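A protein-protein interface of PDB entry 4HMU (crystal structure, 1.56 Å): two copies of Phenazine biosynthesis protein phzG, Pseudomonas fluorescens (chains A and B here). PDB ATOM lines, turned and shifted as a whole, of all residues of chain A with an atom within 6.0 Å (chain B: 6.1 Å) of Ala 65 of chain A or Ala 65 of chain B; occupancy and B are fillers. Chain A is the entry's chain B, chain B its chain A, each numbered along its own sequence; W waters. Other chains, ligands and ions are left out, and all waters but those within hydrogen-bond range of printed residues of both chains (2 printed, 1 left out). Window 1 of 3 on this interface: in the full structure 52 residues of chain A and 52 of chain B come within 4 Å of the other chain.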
ATOM      1  N   ALA A  63      -9.904 -11.996  28.348  1.00  0.00           N
ATOM      2  CA  ALA A  63      -9.768 -10.674  27.766  1.00  0.00           C
ATOM      3  C   ALA A  63      -8.310 -10.278  27.915  1.00  0.00           C
ATOM      4  O   ALA A  63      -7.861  -9.911  29.000  1.00  0.00           O
ATOM      5  CB  ALA A  63     -10.689  -9.666  28.454  1.00  0.00           C
ATOM      6  N   LEU A  64      -7.577 -10.376  26.814  1.00  0.00           N
ATOM      7  CA  LEU A  64      -6.129 -10.240  26.836  1.00  0.00           C
ATOM      8  C   LEU A  64      -5.715  -8.856  26.372  1.00  0.00           C
ATOM      9  O   LEU A  64      -6.063  -8.448  25.255  1.00  0.00           O
ATOM     10  CB  LEU A  64      -5.496 -11.277  25.903  1.00  0.00           C
ATOM     11  CG  LEU A  64      -3.972 -11.201  25.776  1.00  0.00           C
ATOM     12  CD1 LEU A  64      -3.316 -11.672  27.072  1.00  0.00           C
ATOM     13  CD2 LEU A  64      -3.481 -12.002  24.577  1.00  0.00           C
ATOM     14  N   ALA A  65      -4.960  -8.153  27.219  1.00  0.00           N
ATOM     15  CA  ALA A  65      -4.413  -6.837  26.899  1.00  0.00           C
ATOM     16  C   ALA A  65      -2.926  -6.896  26.573  1.00  0.00           C
ATOM     17  O   ALA A  65      -2.140  -7.518  27.293  1.00  0.00           O
ATOM     18  CB  ALA A  65      -4.631  -5.877  28.059  1.00  0.00           C
ATOM     19  N   THR A  66      -2.565  -6.229  25.482  1.00  0.00           N
ATOM     20  CA  THR A  66      -1.179  -6.031  25.087  1.00  0.00           C
ATOM     21  C   THR A  66      -0.997  -4.522  24.927  1.00  0.00           C
ATOM     22  O   THR A  66      -1.966  -3.772  25.049  1.00  0.00           O
ATOM     23  CB  THR A  66      -0.864  -6.762  23.766  1.00  0.00           C
ATOM     24  OG1 THR A  66      -1.789  -6.348  22.751  1.00  0.00           O
ATOM     25  CG2 THR A  66      -0.995  -8.272  23.949  1.00  0.00           C
ATOM     26  N   ALA A  67       0.222  -4.060  24.680  1.00  0.00           N
ATOM     27  CA  ALA A  67       0.424  -2.625  24.460  1.00  0.00           C
ATOM     28  C   ALA A  67       1.383  -2.335  23.314  1.00  0.00           C
ATOM     29  O   ALA A  67       2.315  -3.103  23.052  1.00  0.00           O
ATOM     30  CB  ALA A  67       0.898  -1.948  25.738  1.00  0.00           C
ATOM     31  N   PRO A  73      -2.678   0.511  25.315  1.00  0.00           N
ATOM     32  CA  PRO A  73      -3.216  -0.853  25.342  1.00  0.00           C
ATOM     33  C   PRO A  73      -4.163  -1.165  24.196  1.00  0.00           C
ATOM     34  O   PRO A  73      -4.790  -0.264  23.628  1.00  0.00           O
ATOM     35  CB  PRO A  73      -3.998  -0.910  26.667  1.00  0.00           C
ATOM     36  CG  PRO A  73      -3.517   0.235  27.466  1.00  0.00           C
ATOM     37  CD  PRO A  73      -3.113   1.291  26.487  1.00  0.00           C
ATOM     38  N   SER A  74      -4.241  -2.451  23.873  1.00  0.00           N
ATOM     39  CA  SER A  74      -5.284  -2.999  23.011  1.00  0.00           C
ATOM     40  C   SER A  74      -5.803  -4.275  23.670  1.00  0.00           C
ATOM     41  O   SER A  74      -5.076  -4.916  24.427  1.00  0.00           O
ATOM     42  CB  SER A  74      -4.757  -3.286  21.601  1.00  0.00           C
ATOM     43  OG  SER A  74      -3.710  -4.233  21.616  1.00  0.00           O
ATOM     44  N   THR A  75      -7.051  -4.643  23.390  1.00  0.00           N
ATOM     45  CA  THR A  75      -7.677  -5.795  24.033  1.00  0.00           C
ATOM     46  C   THR A  75      -8.476  -6.609  23.019  1.00  0.00           C
ATOM     47  O   THR A  75      -8.868  -6.099  21.973  1.00  0.00           O
ATOM     48  CB  THR A  75      -8.639  -5.364  25.154  1.00  0.00           C
ATOM     49  OG1 THR A  75      -9.618  -4.456  24.631  1.00  0.00           O
ATOM     50  CG2 THR A  75      -7.890  -4.718  26.309  1.00  0.00           C
ATOM     51  N   ARG A  76      -8.674  -7.885  23.336  1.00  0.00           N
ATOM     52  CA  ARG A  76      -9.525  -8.801  22.582  1.00  0.00           C
ATOM     53  C   ARG A  76      -9.670 -10.076  23.393  1.00  0.00           C
ATOM     54  O   ARG A  76      -8.879 -10.339  24.286  1.00  0.00           O
ATOM     55  CB  ARG A  76      -8.930  -9.159  21.215  1.00  0.00           C
ATOM     56  CG  ARG A  76      -7.769 -10.144  21.255  1.00  0.00           C
ATOM     57  CD  ARG A  76      -6.547  -9.547  21.933  1.00  0.00           C
ATOM     58  NE  ARG A  76      -6.005  -8.460  21.132  1.00  0.00           N
ATOM     59  CZ  ARG A  76      -5.065  -7.611  21.531  1.00  0.00           C
ATOM     60  NH1 ARG A  76      -4.637  -6.680  20.691  1.00  0.00           N
ATOM     61  NH2 ARG A  76      -4.553  -7.678  22.762  1.00  0.00           N
ATOM     62  N   LEU A 102       3.144  -8.091  21.115  1.00  0.00           N
ATOM     63  CA  LEU A 102       3.876  -8.984  22.019  1.00  0.00           C
ATOM     64  C   LEU A 102       5.324  -9.238  21.604  1.00  0.00           C
ATOM     65  O   LEU A 102       6.194  -9.467  22.449  1.00  0.00           O
ATOM     66  CB  LEU A 102       3.159 -10.330  22.140  1.00  0.00           C
ATOM     67  CG  LEU A 102       1.885 -10.293  22.970  1.00  0.00           C
ATOM     68  CD1 LEU A 102       1.147 -11.611  22.852  1.00  0.00           C
ATOM     69  CD2 LEU A 102       2.215  -9.970  24.427  1.00  0.00           C
ATOM     70  N   TRP A 107       5.090  -7.884  27.724  1.00  0.00           N
ATOM     71  CA  TRP A 107       4.230  -7.765  28.898  1.00  0.00           C
ATOM     72  C   TRP A 107       2.755  -7.729  28.507  1.00  0.00           C
ATOM     73  O   TRP A 107       2.349  -6.997  27.591  1.00  0.00           O
ATOM     74  CB  TRP A 107       4.596  -6.527  29.717  1.00  0.00           C
ATOM     75  CG  TRP A 107       5.852  -6.716  30.514  1.00  0.00           C
ATOM     76  CD1 TRP A 107       7.123  -6.375  30.142  1.00  0.00           C
ATOM     77  CD2 TRP A 107       5.959  -7.314  31.811  1.00  0.00           C
ATOM     78  NE1 TRP A 107       8.010  -6.719  31.135  1.00  0.00           N
ATOM     79  CE2 TRP A 107       7.320  -7.292  32.170  1.00  0.00           C
ATOM     80  CE3 TRP A 107       5.034  -7.856  32.707  1.00  0.00           C
ATOM     81  CZ2 TRP A 107       7.775  -7.790  33.390  1.00  0.00           C
ATOM     82  CZ3 TRP A 107       5.492  -8.349  33.922  1.00  0.00           C
ATOM     83  CH2 TRP A 107       6.848  -8.312  34.248  1.00  0.00           C
ATOM     84  N   ALA A 108       1.953  -8.521  29.213  1.00  0.00           N
ATOM     85  CA  ALA A 108       0.535  -8.585  28.931  1.00  0.00           C
ATOM     86  C   ALA A 108      -0.243  -8.840  30.213  1.00  0.00           C
ATOM     87  O   ALA A 108       0.321  -9.210  31.240  1.00  0.00           O
ATOM     88  CB  ALA A 108       0.254  -9.678  27.917  1.00  0.00           C
ATOM     89  N   SER A 109      -1.548  -8.620  30.136  1.00  0.00           N
ATOM     90  CA  SER A 109      -2.446  -8.878  31.241  1.00  0.00           C
ATOM     91  C   SER A 109      -3.753  -9.394  30.677  1.00  0.00           C
ATOM     92  O   SER A 109      -4.247  -8.865  29.682  1.00  0.00           O
ATOM     93  CB  SER A 109      -2.713  -7.589  32.010  1.00  0.00           C
ATOM     94  OG  SER A 109      -3.601  -7.819  33.076  1.00  0.00           O
ATOM     95  N   GLY A 110      -4.330 -10.402  31.313  1.00  0.00           N
ATOM     96  CA  GLY A 110      -5.644 -10.859  30.906  1.00  0.00           C
ATOM     97  C   GLY A 110      -6.575 -11.062  32.086  1.00  0.00           C
ATOM     98  O   GLY A 110      -6.136 -11.370  33.195  1.00  0.00           O
ATOM     99  N   ALA B  63     -13.934  -5.327  30.228  1.00  0.00           N
ATOM    100  CA  ALA B  63     -12.590  -5.694  30.625  1.00  0.00           C
ATOM    101  C   ALA B  63     -11.683  -4.553  30.196  1.00  0.00           C
ATOM    102  O   ALA B  63     -11.370  -4.404  29.012  1.00  0.00           O
ATOM    103  CB  ALA B  63     -12.167  -7.002  29.972  1.00  0.00           C
ATOM    104  N   LEU B  64     -11.280  -3.740  31.169  1.00  0.00           N
ATOM    105  CA  LEU B  64     -10.583  -2.490  30.908  1.00  0.00           C
ATOM    106  C   LEU B  64      -9.094  -2.616  31.168  1.00  0.00           C
ATOM    107  O   LEU B  64      -8.678  -3.009  32.270  1.00  0.00           O
ATOM    108  CB  LEU B  64     -11.153  -1.386  31.803  1.00  0.00           C
ATOM    109  CG  LEU B  64     -10.442  -0.035  31.701  1.00  0.00           C
ATOM    110  CD1 LEU B  64     -10.836   0.644  30.398  1.00  0.00           C
ATOM    111  CD2 LEU B  64     -10.761   0.845  32.915  1.00  0.00           C
ATOM    112  N   ALA B  65      -8.314  -2.300  30.142  1.00  0.00           N
ATOM    113  CA  ALA B  65      -6.863  -2.346  30.199  1.00  0.00           C
ATOM    114  C   ALA B  65      -6.271  -0.942  30.261  1.00  0.00           C
ATOM    115  O   ALA B  65      -6.669  -0.036  29.513  1.00  0.00           O
ATOM    116  CB  ALA B  65      -6.304  -3.096  28.984  1.00  0.00           C
ATOM    117  N   THR B  66      -5.324  -0.789  31.182  1.00  0.00           N
ATOM    118  CA  THR B  66      -4.514   0.401  31.328  1.00  0.00           C
ATOM    119  C   THR B  66      -3.059  -0.074  31.312  1.00  0.00           C
ATOM    120  O   THR B  66      -2.806  -1.277  31.259  1.00  0.00           O
ATOM    121  CB  THR B  66      -4.851   1.126  32.652  1.00  0.00           C
ATOM    122  OG1 THR B  66      -4.710   0.236  33.760  1.00  0.00           O
ATOM    123  CG2 THR B  66      -6.288   1.632  32.646  1.00  0.00           C
ATOM    124  N   ALA B  67      -2.094   0.841  31.338  1.00  0.00           N
ATOM    125  CA  ALA B  67      -0.694   0.423  31.380  1.00  0.00           C
ATOM    126  C   ALA B  67       0.147   1.360  32.238  1.00  0.00           C
ATOM    127  O   ALA B  67      -0.132   2.553  32.328  1.00  0.00           O
ATOM    128  CB  ALA B  67      -0.121   0.326  29.974  1.00  0.00           C
ATOM    129  N   PRO B  73       0.734  -3.724  30.660  1.00  0.00           N
ATOM    130  CA  PRO B  73      -0.718  -3.665  30.853  1.00  0.00           C
ATOM    131  C   PRO B  73      -1.186  -4.251  32.182  1.00  0.00           C
ATOM    132  O   PRO B  73      -0.535  -5.135  32.764  1.00  0.00           O
ATOM    133  CB  PRO B  73      -1.260  -4.528  29.699  1.00  0.00           C
ATOM    134  CG  PRO B  73      -0.174  -4.555  28.701  1.00  0.00           C
ATOM    135  CD  PRO B  73       1.090  -4.556  29.499  1.00  0.00           C
ATOM    136  N   SER B  74      -2.322  -3.746  32.653  1.00  0.00           N
ATOM    137  CA  SER B  74      -3.093  -4.380  33.716  1.00  0.00           C
ATOM    138  C   SER B  74      -4.561  -4.364  33.291  1.00  0.00           C
ATOM    139  O   SER B  74      -4.962  -3.529  32.491  1.00  0.00           O
ATOM    140  CB  SER B  74      -2.917  -3.650  35.045  1.00  0.00           C
ATOM    141  OG  SER B  74      -3.348  -2.312  34.966  1.00  0.00           O
ATOM    142  N   THR B  75      -5.346  -5.296  33.819  1.00  0.00           N
ATOM    143  CA  THR B  75      -6.749  -5.436  33.450  1.00  0.00           C
ATOM    144  C   THR B  75      -7.618  -5.703  34.670  1.00  0.00           C
ATOM    145  O   THR B  75      -7.134  -6.136  35.718  1.00  0.00           O
ATOM    146  CB  THR B  75      -6.973  -6.600  32.467  1.00  0.00           C
ATOM    147  OG1 THR B  75      -6.465  -7.818  33.038  1.00  0.00           O
ATOM    148  CG2 THR B  75      -6.297  -6.326  31.141  1.00  0.00           C
ATOM    149  N   ARG B  76      -8.907  -5.426  34.507  1.00  0.00           N
ATOM    150  CA  ARG B  76      -9.935  -5.742  35.488  1.00  0.00           C
ATOM    151  C   ARG B  76     -11.277  -5.427  34.842  1.00  0.00           C
ATOM    152  O   ARG B  76     -11.331  -4.716  33.842  1.00  0.00           O
ATOM    153  CB  ARG B  76      -9.782  -4.904  36.757  1.00  0.00           C
ATOM    154  CG  ARG B  76     -10.221  -3.455  36.615  1.00  0.00           C
ATOM    155  CD  ARG B  76      -9.303  -2.684  35.686  1.00  0.00           C
ATOM    156  NE  ARG B  76      -7.981  -2.515  36.283  1.00  0.00           N
ATOM    157  CZ  ARG B  76      -6.915  -2.051  35.645  1.00  0.00           C
ATOM    158  NH1 ARG B  76      -5.773  -1.902  36.301  1.00  0.00           N
ATOM    159  NH2 ARG B  76      -6.985  -1.721  34.363  1.00  0.00           N
ATOM    160  N   GLU B 101      -2.601   4.497  37.026  1.00  0.00           N
ATOM    161  CA  GLU B 101      -2.081   4.302  35.678  1.00  0.00           C
ATOM    162  C   GLU B 101      -2.667   5.329  34.714  1.00  0.00           C
ATOM    163  O   GLU B 101      -1.939   5.918  33.921  1.00  0.00           O
ATOM    164  CB  GLU B 101      -2.287   2.853  35.206  1.00  0.00           C
ATOM    165  CG  GLU B 101      -1.409   1.892  36.015  1.00  0.00           C
ATOM    166  CD  GLU B 101      -1.368   0.461  35.506  1.00  0.00           C
ATOM    167  OE1 GLU B 101      -2.115   0.101  34.563  1.00  0.00           O
ATOM    168  OE2 GLU B 101      -0.558  -0.315  36.072  1.00  0.00           O
ATOM    169  N   LEU B 102      -3.969   5.576  34.794  1.00  0.00           N
ATOM    170  CA  LEU B 102      -4.598   6.542  33.893  1.00  0.00           C
ATOM    171  C   LEU B 102      -4.129   7.973  34.129  1.00  0.00           C
ATOM    172  O   LEU B 102      -4.127   8.793  33.202  1.00  0.00           O
ATOM    173  CB  LEU B 102      -6.117   6.476  34.009  1.00  0.00           C
ATOM    174  CG  LEU B 102      -6.724   5.212  33.402  1.00  0.00           C
ATOM    175  CD1 LEU B 102      -8.198   5.117  33.765  1.00  0.00           C
ATOM    176  CD2 LEU B 102      -6.528   5.202  31.886  1.00  0.00           C
ATOM    177  N   TRP B 107      -4.065   6.489  27.916  1.00  0.00           N
ATOM    178  CA  TRP B 107      -4.512   5.528  26.910  1.00  0.00           C
ATOM    179  C   TRP B 107      -5.003   4.228  27.526  1.00  0.00           C
ATOM    180  O   TRP B 107      -4.350   3.645  28.397  1.00  0.00           O
ATOM    181  CB  TRP B 107      -3.419   5.265  25.873  1.00  0.00           C
ATOM    182  CG  TRP B 107      -3.222   6.429  24.970  1.00  0.00           C
ATOM    183  CD1 TRP B 107      -2.360   7.476  25.152  1.00  0.00           C
ATOM    184  CD2 TRP B 107      -3.911   6.687  23.738  1.00  0.00           C
ATOM    185  NE1 TRP B 107      -2.469   8.365  24.107  1.00  0.00           N
ATOM    186  CE2 TRP B 107      -3.411   7.901  23.227  1.00  0.00           C
ATOM    187  CE3 TRP B 107      -4.895   6.004  23.020  1.00  0.00           C
ATOM    188  CZ2 TRP B 107      -3.861   8.445  22.026  1.00  0.00           C
ATOM    189  CZ3 TRP B 107      -5.342   6.547  21.825  1.00  0.00           C
ATOM    190  CH2 TRP B 107      -4.827   7.756  21.342  1.00  0.00           C
ATOM    191  N   ALA B 108      -6.162   3.782  27.051  1.00  0.00           N
ATOM    192  CA  ALA B 108      -6.806   2.589  27.571  1.00  0.00           C
ATOM    193  C   ALA B 108      -7.525   1.851  26.463  1.00  0.00           C
ATOM    194  O   ALA B 108      -7.743   2.389  25.379  1.00  0.00           O
ATOM    195  CB  ALA B 108      -7.783   2.959  28.695  1.00  0.00           C
ATOM    196  N   SER B 109      -7.879   0.606  26.747  1.00  0.00           N
ATOM    197  CA  SER B 109      -8.656  -0.203  25.832  1.00  0.00           C
ATOM    198  C   SER B 109      -9.543  -1.103  26.649  1.00  0.00           C
ATOM    199  O   SER B 109      -9.114  -1.623  27.673  1.00  0.00           O
ATOM    200  CB  SER B 109      -7.738  -1.059  24.964  1.00  0.00           C
ATOM    201  OG  SER B 109      -8.497  -1.896  24.113  1.00  0.00           O
ATOM    202  N   GLY B 110     -10.783  -1.275  26.213  1.00  0.00           N
ATOM    203  CA  GLY B 110     -11.672  -2.211  26.867  1.00  0.00           C
ATOM    204  C   GLY B 110     -12.401  -3.109  25.891  1.00  0.00           C
ATOM    205  O   GLY B 110     -12.673  -2.708  24.764  1.00  0.00           O
HETATM  206  O   HOH W   1      -5.246   2.469  23.818  1.00  0.00           O
HETATM  207  O   HOH W   2       1.637  -6.838  32.383  1.00  0.00           O
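The backbone NH (N) of Ala 65 of chain B lies within hydrogen-bond range of the backbone carbonyl oxygen (O) of Ser 109 of chain B (2.7 Å). O of Thr 66 of chain B lies within hydrogen-bond range of N of Ser 74 of chain B (2.9 Å). OG1 of Thr 66 of chain B sits at hydrogen-bond distance from NH2 of Arg 76 of chain B (3.1 Å). OG of Ser 74 of chain B lies within hydrogen-bond range of NH1 of Arg 76 of chain B. The side-chain hydroxyl (OG) of Ser 74 of chain B sits at hydrogen-bond distance from the side-chain carboxylate (OE1) of Glu 101 of chain B, at 2.7 Å. The backbone NH (N) of Ser 74 of chain A sits at hydrogen-bond distance from the backbone carbonyl oxygen (O) of Thr 66 of chain A.
Printed residues of chain B within 4 Å of Ala 65 of chain A: Ala 65, Pro 73 and Thr 75. Of chain A, only Ala 65, Pro 73 and Thr 75 come within 4 Å of Ala 65 of chain B. Of the printed residues of chain B, Ser 109 of chain A touches Pro 73, Ser 74 and Thr 75. Printed residues of chain A within 4 Å of Trp 107 of chain B: Pro 73 (3.3 Å). Of the printed residues of chain B, Gly 110 of chain A touches Thr 75 (3.4 Å). Of the printed residues of chain A, Ala 108 of chain B touches Pro 73 (3.98 Å). Printed residues of chain B within 4 Å of Ala 63 of chain A: Ala 63 (3.4 Å). The nearest residue of chain A that does not touch Ala 65 of chain B is Ser 74 of chain A (5.1 Å). The nearest printed residue of chain A that does not touch Ser 74 of chain B is Ala 65 of chain A (5.0 Å).
Ala 65 of chain A touches Thr 75 of chain B, and with the chains exchanged Thr 75 of chain A touches Ala 65 of chain B. Pro 73 of chain A touches Ala 108 of chain B, but with the chains exchanged Ala 108 of chain A does not touch Pro 73 of chain B (4.1 Å). Ser 74 of chain A touches Ser 109 of chain B, and with the chains exchanged Ser 109 of chain A touches Ser 74 of chain B. Thr 75 of chain A touches Gly 110 of chain B, and with the chains exchanged Gly 110 of chain A touches Thr 75 of chain B. Of the 19 pairs that touch across the chains among the printed residues, 18 have their exchanged pair printed and touching as well.
Water W1 lies within hydrogen-bond range of the backbone carbonyl oxygen (O) of Pro 73 of chain A (2.8 Å) and the backbone carbonyl oxygen (O) of Ala 108 of chain B (2.9 Å). Water W2 bridges O of Pro 73 of chain B and O of Ala 108 of chain A.
Hydrophobic or aromatic side chains of chain B that line the printed part of chain A: Ala 63, Ala 65 and Pro 73. Hydrophobic or aromatic side chains of chain A within 4 Å of the printed part of chain B: Ala 63, Ala 65 and Pro 73. Among the printed residues, 19 pairs touch across the chains.
The side-chain hydroxyl (OG1) of Thr 75 of chain B is in hydrogen-bond range of the side-chain hydroxyl (OG) of Ser 109 of chain A (2.9 Å). The side-chain hydroxyl of Ser 109 of chain B lies within hydrogen-bond range of the side-chain hydroxyl of Thr 75 of chain A (2.8 Å).
Ala 65 of chain B touches Ala 65 of chain A (CB to CB, 3.4 Å). O of Ala 65 of chain A touches CG of Pro 73 of chain B, 3.8 Å away. Thr 66 of chain A touches Pro 73 of chain B. C of Thr 66 of chain B touches CG of Pro 73 of chain A (3.9 Å). Ala 108 of chain B touches Pro 73 of chain A (N to CD, 3.98 Å). Ser 74 of chain A touches Ser 109 of chain B. Thr 75 of chain A touches Gly 110 of chain B. Pro 73 of chain B touches Trp 107 of chain A (CD to O, 3.3 Å). Ser 109 of chain A touches Ser 74 of chain B. Thr 75 of chain B touches Gly 110 of chain A.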
